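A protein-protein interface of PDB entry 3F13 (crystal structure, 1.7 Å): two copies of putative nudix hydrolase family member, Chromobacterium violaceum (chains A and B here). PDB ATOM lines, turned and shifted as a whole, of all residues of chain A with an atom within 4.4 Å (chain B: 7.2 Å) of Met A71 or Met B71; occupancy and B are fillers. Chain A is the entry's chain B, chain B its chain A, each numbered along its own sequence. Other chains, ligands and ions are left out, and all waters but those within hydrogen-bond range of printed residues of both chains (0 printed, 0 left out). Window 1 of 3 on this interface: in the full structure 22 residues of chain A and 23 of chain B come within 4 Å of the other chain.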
ATOM      1  N   SER A  53      -1.106   2.844 -29.560  1.00  0.00           N
ATOM      2  CA  SER A  53      -1.477   3.160 -28.188  1.00  0.00           C
ATOM      3  C   SER A  53      -1.295   4.664 -27.993  1.00  0.00           C
ATOM      4  O   SER A  53      -2.055   5.267 -27.261  1.00  0.00           O
ATOM      5  CB  SER A  53      -0.605   2.391 -27.210  1.00  0.00           C
ATOM      6  OG  SER A  53       0.756   2.562 -27.549  1.00  0.00           O
ATOM      7  N   LEU A  56      -4.237   6.311 -29.755  1.00  0.00           N
ATOM      8  CA  LEU A  56      -5.503   6.144 -29.029  1.00  0.00           C
ATOM      9  C   LEU A  56      -5.708   7.298 -28.017  1.00  0.00           C
ATOM     10  O   LEU A  56      -6.780   7.910 -27.945  1.00  0.00           O
ATOM     11  CB  LEU A  56      -5.554   4.794 -28.310  1.00  0.00           C
ATOM     12  CG  LEU A  56      -7.066   4.547 -27.961  1.00  0.00           C
ATOM     13  CD1 LEU A  56      -7.903   4.919 -29.212  1.00  0.00           C
ATOM     14  CD2 LEU A  56      -7.460   3.187 -27.535  1.00  0.00           C
ATOM     15  N   ILE A  57      -4.685   7.571 -27.220  1.00  0.00           N
ATOM     16  CA  ILE A  57      -4.798   8.639 -26.226  1.00  0.00           C
ATOM     17  C   ILE A  57      -5.091  10.006 -26.863  1.00  0.00           C
ATOM     18  O   ILE A  57      -5.958  10.755 -26.420  1.00  0.00           O
ATOM     19  CB  ILE A  57      -3.545   8.695 -25.328  1.00  0.00           C
ATOM     20  CG1 ILE A  57      -3.375   7.370 -24.592  1.00  0.00           C
ATOM     21  CG2 ILE A  57      -3.692   9.824 -24.339  1.00  0.00           C
ATOM     22  CD1 ILE A  57      -1.943   7.193 -24.005  1.00  0.00           C
ATOM     23  N   ASN A  69      -5.642   7.520 -18.604  1.00  0.00           N
ATOM     24  CA  ASN A  69      -4.582   7.177 -17.596  1.00  0.00           C
ATOM     25  C   ASN A  69      -4.132   5.715 -17.610  1.00  0.00           C
ATOM     26  O   ASN A  69      -3.040   5.333 -17.124  1.00  0.00           O
ATOM     27  CB  ASN A  69      -5.015   7.536 -16.124  1.00  0.00           C
ATOM     28  CG  ASN A  69      -6.396   6.905 -15.639  1.00  0.00           C
ATOM     29  OD1 ASN A  69      -6.465   5.868 -14.904  1.00  0.00           O
ATOM     30  ND2 ASN A  69      -7.481   7.634 -15.923  1.00  0.00           N
ATOM     31  N   SER A  70      -5.053   4.875 -18.055  1.00  0.00           N
ATOM     32  CA  SER A  70      -4.904   3.415 -18.038  1.00  0.00           C
ATOM     33  C   SER A  70      -5.627   2.816 -19.241  1.00  0.00           C
ATOM     34  O   SER A  70      -6.745   3.252 -19.616  1.00  0.00           O
ATOM     35  CB  SER A  70      -5.524   2.874 -16.751  1.00  0.00           C
ATOM     36  OG  SER A  70      -4.926   3.522 -15.618  1.00  0.00           O
ATOM     37  N   MET A  71      -4.993   1.823 -19.838  1.00  0.00           N
ATOM     38  CA  MET A  71      -5.522   1.145 -21.006  1.00  0.00           C
ATOM     39  C   MET A  71      -5.061  -0.301 -20.971  1.00  0.00           C
ATOM     40  O   MET A  71      -3.943  -0.612 -20.531  1.00  0.00           O
ATOM     41  CB  MET A  71      -4.964   1.840 -22.283  1.00  0.00           C
ATOM     42  CG  MET A  71      -3.368   2.427 -22.219  1.00  0.00           C
ATOM     43  SD  MET A  71      -2.936   2.973 -23.885  1.00  0.00           S
ATOM     44  CE  MET A  71      -4.551   2.955 -24.661  1.00  0.00           C
ATOM     45  N   LEU A  72      -5.871  -1.189 -21.508  1.00  0.00           N
ATOM     46  CA  LEU A  72      -5.472  -2.572 -21.624  1.00  0.00           C
ATOM     47  C   LEU A  72      -5.675  -3.034 -23.064  1.00  0.00           C
ATOM     48  O   LEU A  72      -6.809  -3.038 -23.557  1.00  0.00           O
ATOM     49  CB  LEU A  72      -6.305  -3.446 -20.670  1.00  0.00           C
ATOM     50  CG  LEU A  72      -6.112  -4.940 -20.886  1.00  0.00           C
ATOM     51  CD1 LEU A  72      -4.646  -5.306 -20.514  1.00  0.00           C
ATOM     52  CD2 LEU A  72      -7.107  -5.717 -20.043  1.00  0.00           C
ATOM     53  N   TYR A  73      -4.601  -3.387 -23.754  1.00  0.00           N
ATOM     54  CA  TYR A  73      -4.723  -3.948 -25.110  1.00  0.00           C
ATOM     55  C   TYR A  73      -5.527  -5.255 -25.082  1.00  0.00           C
ATOM     56  O   TYR A  73      -5.185  -6.189 -24.351  1.00  0.00           O
ATOM     57  CB  TYR A  73      -3.332  -4.163 -25.757  1.00  0.00           C
ATOM     58  CG  TYR A  73      -3.361  -5.051 -26.986  1.00  0.00           C
ATOM     59  CD1 TYR A  73      -3.917  -4.598 -28.183  1.00  0.00           C
ATOM     60  CD2 TYR A  73      -2.936  -6.377 -26.921  1.00  0.00           C
ATOM     61  CE1 TYR A  73      -3.995  -5.433 -29.309  1.00  0.00           C
ATOM     62  CE2 TYR A  73      -2.984  -7.220 -28.044  1.00  0.00           C
ATOM     63  CZ  TYR A  73      -3.531  -6.723 -29.234  1.00  0.00           C
ATOM     64  OH  TYR A  73      -3.594  -7.511 -30.360  1.00  0.00           O
ATOM     65  N   TYR A  87      -8.509  -1.423 -27.387  1.00  0.00           N
ATOM     66  CA  TYR A  87      -8.077  -1.257 -25.985  1.00  0.00           C
ATOM     67  C   TYR A  87      -9.242  -0.891 -25.069  1.00  0.00           C
ATOM     68  O   TYR A  87     -10.068  -0.025 -25.419  1.00  0.00           O
ATOM     69  CB  TYR A  87      -7.102  -0.080 -25.829  1.00  0.00           C
ATOM     70  CG  TYR A  87      -5.929  -0.084 -26.790  1.00  0.00           C
ATOM     71  CD1 TYR A  87      -4.671  -0.522 -26.368  1.00  0.00           C
ATOM     72  CD2 TYR A  87      -6.076   0.337 -28.116  1.00  0.00           C
ATOM     73  CE1 TYR A  87      -3.585  -0.540 -27.209  1.00  0.00           C
ATOM     74  CE2 TYR A  87      -4.953   0.340 -28.988  1.00  0.00           C
ATOM     75  CZ  TYR A  87      -3.724  -0.143 -28.522  1.00  0.00           C
ATOM     76  OH  TYR A  87      -2.599  -0.140 -29.353  1.00  0.00           O
ATOM     77  N   LEU A  88      -9.256  -1.454 -23.873  1.00  0.00           N
ATOM     78  CA  LEU A  88     -10.224  -1.069 -22.838  1.00  0.00           C
ATOM     79  C   LEU A  88      -9.543   0.082 -22.114  1.00  0.00           C
ATOM     80  O   LEU A  88      -8.400  -0.071 -21.662  1.00  0.00           O
ATOM     81  CB  LEU A  88     -10.418  -2.213 -21.843  1.00  0.00           C
ATOM     82  CG  LEU A  88     -11.347  -1.889 -20.652  1.00  0.00           C
ATOM     83  CD1 LEU A  88     -12.791  -1.679 -21.082  1.00  0.00           C
ATOM     84  CD2 LEU A  88     -11.299  -3.004 -19.594  1.00  0.00           C
ATOM     85  N   CYS A  89     -10.189   1.235 -22.061  1.00  0.00           N
ATOM     86  CA  CYS A  89      -9.580   2.427 -21.446  1.00  0.00           C
ATOM     87  C   CYS A  89     -10.360   2.975 -20.256  1.00  0.00           C
ATOM     88  O   CYS A  89     -11.580   2.981 -20.271  1.00  0.00           O
ATOM     89  CB  CYS A  89      -9.480   3.545 -22.473  1.00  0.00           C
ATOM     90  SG  CYS A  89      -8.715   3.073 -24.049  1.00  0.00           S
ATOM     91  N   ALA B  19       6.552  11.508 -16.226  1.00  0.00           N
ATOM     92  CA  ALA B  19       5.839  10.255 -16.351  1.00  0.00           C
ATOM     93  C   ALA B  19       6.902   9.196 -16.087  1.00  0.00           C
ATOM     94  O   ALA B  19       7.999   9.243 -16.660  1.00  0.00           O
ATOM     95  CB  ALA B  19       5.239  10.076 -17.746  1.00  0.00           C
ATOM     96  N   THR B  20       6.590   8.249 -15.215  1.00  0.00           N
ATOM     97  CA  THR B  20       7.554   7.214 -14.897  1.00  0.00           C
ATOM     98  C   THR B  20       6.923   5.829 -15.035  1.00  0.00           C
ATOM     99  O   THR B  20       5.735   5.636 -14.689  1.00  0.00           O
ATOM    100  CB  THR B  20       8.127   7.437 -13.464  1.00  0.00           C
ATOM    101  OG1 THR B  20       8.786   8.738 -13.392  1.00  0.00           O
ATOM    102  CG2 THR B  20       9.092   6.366 -13.118  1.00  0.00           C
ATOM    103  N   ALA B  21       7.713   4.887 -15.560  1.00  0.00           N
ATOM    104  CA  ALA B  21       7.216   3.561 -15.942  1.00  0.00           C
ATOM    105  C   ALA B  21       7.778   2.485 -15.047  1.00  0.00           C
ATOM    106  O   ALA B  21       8.990   2.444 -14.830  1.00  0.00           O
ATOM    107  CB  ALA B  21       7.562   3.270 -17.410  1.00  0.00           C
ATOM    108  N   ARG B  52       0.812  13.191 -19.581  1.00  0.00           N
ATOM    109  CA  ARG B  52       1.937  12.387 -19.150  1.00  0.00           C
ATOM    110  C   ARG B  52       1.816  10.975 -19.763  1.00  0.00           C
ATOM    111  O   ARG B  52       2.816  10.365 -20.087  1.00  0.00           O
ATOM    112  CB  ARG B  52       1.975  12.303 -17.614  1.00  0.00           C
ATOM    113  CG  ARG B  52       2.484  13.545 -16.868  1.00  0.00           C
ATOM    114  CD  ARG B  52       2.243  13.221 -15.404  1.00  0.00           C
ATOM    115  NE  ARG B  52       2.732  14.165 -14.405  1.00  0.00           N
ATOM    116  CZ  ARG B  52       1.992  15.171 -13.942  1.00  0.00           C
ATOM    117  NH1 ARG B  52       0.814  15.439 -14.496  1.00  0.00           N
ATOM    118  NH2 ARG B  52       2.460  15.958 -12.977  1.00  0.00           N
ATOM    119  N   SER B  53       0.604  10.468 -19.954  1.00  0.00           N
ATOM    120  CA  SER B  53       0.476   9.106 -20.505  1.00  0.00           C
ATOM    121  C   SER B  53       1.015   9.048 -21.962  1.00  0.00           C
ATOM    122  O   SER B  53       1.680   8.070 -22.355  1.00  0.00           O
ATOM    123  CB  SER B  53      -0.978   8.611 -20.396  1.00  0.00           C
ATOM    124  OG  SER B  53      -1.841   9.531 -21.054  1.00  0.00           O
ATOM    125  N   GLN B  54       0.776  10.104 -22.743  1.00  0.00           N
ATOM    126  CA  GLN B  54       1.319  10.209 -24.099  1.00  0.00           C
ATOM    127  C   GLN B  54       2.833  10.278 -24.098  1.00  0.00           C
ATOM    128  O   GLN B  54       3.518   9.651 -24.897  1.00  0.00           O
ATOM    129  CB  GLN B  54       0.814  11.486 -24.764  1.00  0.00           C
ATOM    130  CG  GLN B  54      -0.648  11.494 -25.006  1.00  0.00           C
ATOM    131  CD  GLN B  54      -1.106  12.781 -25.653  1.00  0.00           C
ATOM    132  OE1 GLN B  54      -1.378  13.783 -24.970  1.00  0.00           O
ATOM    133  NE2 GLN B  54      -1.188  12.766 -26.984  1.00  0.00           N
ATOM    134  N   LEU B  56       4.830   9.176 -21.821  1.00  0.00           N
ATOM    135  CA  LEU B  56       5.438   7.959 -21.325  1.00  0.00           C
ATOM    136  C   LEU B  56       5.642   6.923 -22.444  1.00  0.00           C
ATOM    137  O   LEU B  56       6.713   6.313 -22.555  1.00  0.00           O
ATOM    138  CB  LEU B  56       4.576   7.347 -20.203  1.00  0.00           C
ATOM    139  CG  LEU B  56       5.414   6.246 -19.541  1.00  0.00           C
ATOM    140  CD1 LEU B  56       6.752   6.817 -19.156  1.00  0.00           C
ATOM    141  CD2 LEU B  56       4.728   5.731 -18.323  1.00  0.00           C
ATOM    142  N   ILE B  57       4.633   6.758 -23.294  1.00  0.00           N
ATOM    143  CA  ILE B  57       4.749   5.757 -24.351  1.00  0.00           C
ATOM    144  C   ILE B  57       5.865   6.160 -25.314  1.00  0.00           C
ATOM    145  O   ILE B  57       6.667   5.338 -25.729  1.00  0.00           O
ATOM    146  CB  ILE B  57       3.460   5.635 -25.147  1.00  0.00           C
ATOM    147  CG1 ILE B  57       2.360   5.047 -24.259  1.00  0.00           C
ATOM    148  CG2 ILE B  57       3.717   4.669 -26.275  1.00  0.00           C
ATOM    149  CD1 ILE B  57       0.935   5.213 -24.848  1.00  0.00           C
ATOM    150  N   ILE B  60       9.444   5.825 -23.315  1.00  0.00           N
ATOM    151  CA  ILE B  60       9.890   4.454 -23.142  1.00  0.00           C
ATOM    152  C   ILE B  60      10.361   3.865 -24.484  1.00  0.00           C
ATOM    153  O   ILE B  60      11.404   3.200 -24.567  1.00  0.00           O
ATOM    154  CB  ILE B  60       8.787   3.602 -22.558  1.00  0.00           C
ATOM    155  CG1 ILE B  60       8.462   4.077 -21.127  1.00  0.00           C
ATOM    156  CG2 ILE B  60       9.161   2.107 -22.670  1.00  0.00           C
ATOM    157  CD1 ILE B  60       9.629   4.030 -20.195  1.00  0.00           C
ATOM    158  N   ILE B  68       4.845   0.174 -25.625  1.00  0.00           N
ATOM    159  CA  ILE B  68       3.817  -0.025 -24.603  1.00  0.00           C
ATOM    160  C   ILE B  68       2.414  -0.225 -25.214  1.00  0.00           C
ATOM    161  O   ILE B  68       2.003   0.576 -26.034  1.00  0.00           O
ATOM    162  CB  ILE B  68       3.839   1.201 -23.645  1.00  0.00           C
ATOM    163  CG1 ILE B  68       5.123   1.151 -22.816  1.00  0.00           C
ATOM    164  CG2 ILE B  68       2.568   1.234 -22.761  1.00  0.00           C
ATOM    165  CD1 ILE B  68       5.281   2.361 -21.878  1.00  0.00           C
ATOM    166  N   ASN B  69       1.713  -1.304 -24.855  1.00  0.00           N
ATOM    167  CA  ASN B  69       0.330  -1.563 -25.286  1.00  0.00           C
ATOM    168  C   ASN B  69      -0.710  -1.496 -24.175  1.00  0.00           C
ATOM    169  O   ASN B  69      -1.907  -1.479 -24.431  1.00  0.00           O
ATOM    170  CB  ASN B  69       0.209  -2.928 -25.995  1.00  0.00           C
ATOM    171  CG  ASN B  69       0.627  -4.132 -25.123  1.00  0.00           C
ATOM    172  OD1 ASN B  69      -0.109  -4.594 -24.220  1.00  0.00           O
ATOM    173  ND2 ASN B  69       1.763  -4.722 -25.475  1.00  0.00           N
ATOM    174  N   SER B  70      -0.233  -1.554 -22.940  1.00  0.00           N
ATOM    175  CA  SER B  70      -1.133  -1.547 -21.788  1.00  0.00           C
ATOM    176  C   SER B  70      -0.407  -0.806 -20.670  1.00  0.00           C
ATOM    177  O   SER B  70       0.831  -0.941 -20.502  1.00  0.00           O
ATOM    178  CB  SER B  70      -1.469  -2.975 -21.322  1.00  0.00           C
ATOM    179  OG  SER B  70      -2.054  -3.781 -22.356  1.00  0.00           O
ATOM    180  N   MET B  71      -1.162  -0.034 -19.903  1.00  0.00           N
ATOM    181  CA  MET B  71      -0.588   0.724 -18.802  1.00  0.00           C
ATOM    182  C   MET B  71      -1.659   0.916 -17.757  1.00  0.00           C
ATOM    183  O   MET B  71      -2.857   1.043 -18.078  1.00  0.00           O
ATOM    184  CB  MET B  71      -0.007   2.072 -19.278  1.00  0.00           C
ATOM    185  CG  MET B  71      -0.963   3.049 -19.984  1.00  0.00           C
ATOM    186  SD  MET B  71      -0.164   4.479 -20.856  1.00  0.00           S
ATOM    187  CE  MET B  71       1.472   4.454 -20.106  1.00  0.00           C
ATOM    188  N   LEU B  72      -1.217   0.933 -16.512  1.00  0.00           N
ATOM    189  CA  LEU B  72      -2.078   1.262 -15.400  1.00  0.00           C
ATOM    190  C   LEU B  72      -1.481   2.353 -14.531  1.00  0.00           C
ATOM    191  O   LEU B  72      -0.401   2.185 -13.975  1.00  0.00           O
ATOM    192  CB  LEU B  72      -2.325   0.008 -14.565  1.00  0.00           C
ATOM    193  CG  LEU B  72      -3.098   0.228 -13.253  1.00  0.00           C
ATOM    194  CD1 LEU B  72      -4.579   0.491 -13.612  1.00  0.00           C
ATOM    195  CD2 LEU B  72      -2.989  -0.965 -12.275  1.00  0.00           C
ATOM    196  N   TYR B  73      -2.189   3.460 -14.414  1.00  0.00           N
ATOM    197  CA  TYR B  73      -1.786   4.569 -13.563  1.00  0.00           C
ATOM    198  C   TYR B  73      -1.867   4.108 -12.117  1.00  0.00           C
ATOM    199  O   TYR B  73      -2.930   3.588 -11.700  1.00  0.00           O
ATOM    200  CB  TYR B  73      -2.770   5.696 -13.742  1.00  0.00           C
ATOM    201  CG  TYR B  73      -2.655   6.683 -12.595  1.00  0.00           C
ATOM    202  CD1 TYR B  73      -1.494   7.433 -12.439  1.00  0.00           C
ATOM    203  CD2 TYR B  73      -3.655   6.778 -11.616  1.00  0.00           C
ATOM    204  CE1 TYR B  73      -1.349   8.350 -11.404  1.00  0.00           C
ATOM    205  CE2 TYR B  73      -3.522   7.691 -10.524  1.00  0.00           C
ATOM    206  CZ  TYR B  73      -2.339   8.455 -10.431  1.00  0.00           C
ATOM    207  OH  TYR B  73      -2.155   9.360  -9.408  1.00  0.00           O
ATOM    208  N   LEU B  74      -0.763   4.263 -11.373  1.00  0.00           N
ATOM    209  CA  LEU B  74      -0.662   3.677 -10.009  1.00  0.00           C
ATOM    210  C   LEU B  74      -0.805   4.742  -8.910  1.00  0.00           C
ATOM    211  O   LEU B  74      -1.645   4.625  -7.986  1.00  0.00           O
ATOM    212  CB  LEU B  74       0.673   2.904  -9.826  1.00  0.00           C
ATOM    213  CG  LEU B  74       0.987   1.798 -10.840  1.00  0.00           C
ATOM    214  CD1 LEU B  74       2.381   1.182 -10.503  1.00  0.00           C
ATOM    215  CD2 LEU B  74      -0.165   0.728 -10.868  1.00  0.00           C
ATOM    216  N   TYR B  87       3.241   4.628 -13.632  1.00  0.00           N
ATOM    217  CA  TYR B  87       2.405   3.685 -14.391  1.00  0.00           C
ATOM    218  C   TYR B  87       3.058   2.304 -14.456  1.00  0.00           C
ATOM    219  O   TYR B  87       4.276   2.198 -14.764  1.00  0.00           O
ATOM    220  CB  TYR B  87       2.206   4.150 -15.834  1.00  0.00           C
ATOM    221  CG  TYR B  87       1.622   5.521 -15.962  1.00  0.00           C
ATOM    222  CD1 TYR B  87       0.270   5.695 -16.268  1.00  0.00           C
ATOM    223  CD2 TYR B  87       2.451   6.644 -15.907  1.00  0.00           C
ATOM    224  CE1 TYR B  87      -0.256   6.961 -16.428  1.00  0.00           C
ATOM    225  CE2 TYR B  87       1.940   7.909 -16.055  1.00  0.00           C
ATOM    226  CZ  TYR B  87       0.588   8.064 -16.338  1.00  0.00           C
ATOM    227  OH  TYR B  87       0.104   9.349 -16.471  1.00  0.00           O
ATOM    228  N   LEU B  88       2.271   1.261 -14.189  1.00  0.00           N
ATOM    229  CA  LEU B  88       2.722  -0.093 -14.527  1.00  0.00           C
ATOM    230  C   LEU B  88       2.470  -0.262 -16.022  1.00  0.00           C
ATOM    231  O   LEU B  88       1.363   0.011 -16.499  1.00  0.00           O
ATOM    232  CB  LEU B  88       1.959  -1.150 -13.730  1.00  0.00           C
ATOM    233  CG  LEU B  88       2.279  -2.569 -14.197  1.00  0.00           C
ATOM    234  CD1 LEU B  88       3.551  -3.043 -13.547  1.00  0.00           C
ATOM    235  CD2 LEU B  88       1.113  -3.451 -13.822  1.00  0.00           C
ATOM    236  N   CYS B  89       3.503  -0.636 -16.768  1.00  0.00           N
ATOM    237  CA  CYS B  89       3.401  -0.783 -18.238  1.00  0.00           C
ATOM    238  C   CYS B  89       3.766  -2.210 -18.676  1.00  0.00           C
ATOM    239  O   CYS B  89       4.691  -2.808 -18.106  1.00  0.00           O
ATOM    240  CB  CYS B  89       4.333   0.204 -18.958  1.00  0.00           C
ATOM    241  SG  CYS B  89       4.068   1.919 -18.471  1.00  0.00           S
ATOM    242  N   ILE B  90       3.059  -2.697 -19.709  1.00  0.00           N
ATOM    243  CA  ILE B  90       3.340  -3.954 -20.399  1.00  0.00           C
ATOM    244  C   ILE B  90       3.689  -3.613 -21.836  1.00  0.00           C
ATOM    245  O   ILE B  90       3.013  -2.779 -22.491  1.00  0.00           O
ATOM    246  CB  ILE B  90       2.110  -4.894 -20.450  1.00  0.00           C
ATOM    247  CG1 ILE B  90       1.408  -4.994 -19.093  1.00  0.00           C
ATOM    248  CG2 ILE B  90       2.495  -6.268 -21.015  1.00  0.00           C
ATOM    249  CD1 ILE B  90       0.441  -6.104 -19.060  1.00  0.00           C
ATOM    250  N   LEU B 144      -2.936  -7.303 -13.700  1.00  0.00           N
ATOM    251  CA  LEU B 144      -2.058  -6.947 -14.810  1.00  0.00           C
ATOM    252  C   LEU B 144      -0.734  -7.711 -14.744  1.00  0.00           C
ATOM    253  O   LEU B 144      -0.222  -8.165 -15.756  1.00  0.00           O
ATOM    254  CB  LEU B 144      -1.829  -5.452 -14.835  1.00  0.00           C
ATOM    255  CG  LEU B 144      -2.927  -4.692 -15.559  1.00  0.00           C
ATOM    256  CD1 LEU B 144      -2.738  -3.217 -15.188  1.00  0.00           C
ATOM    257  CD2 LEU B 144      -2.799  -4.901 -17.092  1.00  0.00           C
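Ile B57 touches Ser A53 (CD1 to OG, 3.8 Å). CD1 of Ile A57 touches OG of Ser B53, 3.8 Å away. Gln B54 touches Ile A57. CD1 of Ile A57 touches CD1 of Ile B57 (3.6 Å). CE1 of Tyr B87 touches O of Asn A69, 3.3 Å away. Ser A70 touches Leu B72 (OG to CA, 3.6 Å). Ser B70 touches Met A71 (CA to O, 3.2 Å). Leu A72 touches Ser B70. Leu A72 touches Leu B144. Tyr A87 touches Asn B69 (CE1 to O, 3.4 Å).
Ser A53 touches Ile B57, and with the chains exchanged Ile A57 touches Ser B53. Ile A57 touches its own counterpart, Ile B57. Asn A69 touches Tyr B73, and with the chains exchanged Tyr A73 touches Asn B69. Asn A69 touches Tyr B87, and with the chains exchanged Tyr A87 touches Asn B69. Of the 17 pairs that touch across the chains among the printed residues, 14 have their exchanged pair printed and touching as well.
N of Tyr B73 lies within hydrogen-bond range of O of Asn A69 (3.4 Å). OG of Ser A53 lies within hydrogen-bond range of O of Ile B68, at 2.8 Å. The backbone carbonyl oxygen (O) of Asn B69 lies close to the backbone NH (N) of Tyr A73 (3.4 Å). The side-chain hydroxyl of Ser B70 is in hydrogen-bond range of the backbone NH of Tyr A73, 2.9 Å away. The backbone carbonyl oxygen (O) of Met B71 sits at hydrogen-bond distance from the backbone NH (N) of Met A71. OG of Ser A70 lies within hydrogen-bond range of N of Tyr B73 (3.0 Å).
Of the printed residues of chain B, Asn A69 touches Tyr B73 (3.4 Å) and Tyr B87 (3.3 Å). Of chain B, only Ser B70 (3.2 Å) and Met B71 (2.9 Å) come within 4 Å of Met A71. Of the printed residues of chain B, Tyr A73 touches Asn B69 and Ser B70. Of the printed residues of chain A, Ser B53 touches Ile A57. Of the printed residues of chain A, Gln B54 touches Ile A57. Of the printed residues of chain A, Ile B57 touches Ser A53 (3.8 Å) and Ile A57 (3.6 Å).
Of the 21 printed residues of chain B, 11 touch a printed residue of chain A. Hydrophobic or aromatic side chains of chain B within 4 Å of the printed part of chain A: Ile B57, Met B71, Leu B72, Tyr B73, Tyr B87 and Leu B144. Along chain B the printed residues that touch a printed residue of chain A span positions 53 to 144. Hydrophobic or aromatic side chains of chain A that line the printed part of chain B: Ile A57, Met A71, Leu A72, Tyr A73 and Tyr A87. Among the printed residues, 17 pairs touch across the chains. Among the printed residues, no Asp or Glu carboxylate lies within 4 Å of a Lys or Arg side-chain nitrogen of the other chain.
The backbone NH (N) of Leu A72 lies within hydrogen-bond range of the backbone carbonyl oxygen (O) of Leu A88. The side-chain sulfur (SG) of Cys B89 lies within hydrogen-bond range of the backbone carbonyl oxygen (O) of Tyr B87 (3.7 Å). The backbone carbonyl oxygen of Leu B88 sits at hydrogen-bond distance from the backbone NH of Leu B72 (2.7 Å). N of Ile B90 is in hydrogen-bond range of O of Ser B70 (2.9 Å). The backbone carbonyl oxygen (O) of Tyr A87 lies within hydrogen-bond range of the side-chain sulfur (SG) of Cys A89, 3.6 Å away. N of Asn B69 lies within hydrogen-bond range of O of Ile B90 (3.1 Å).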
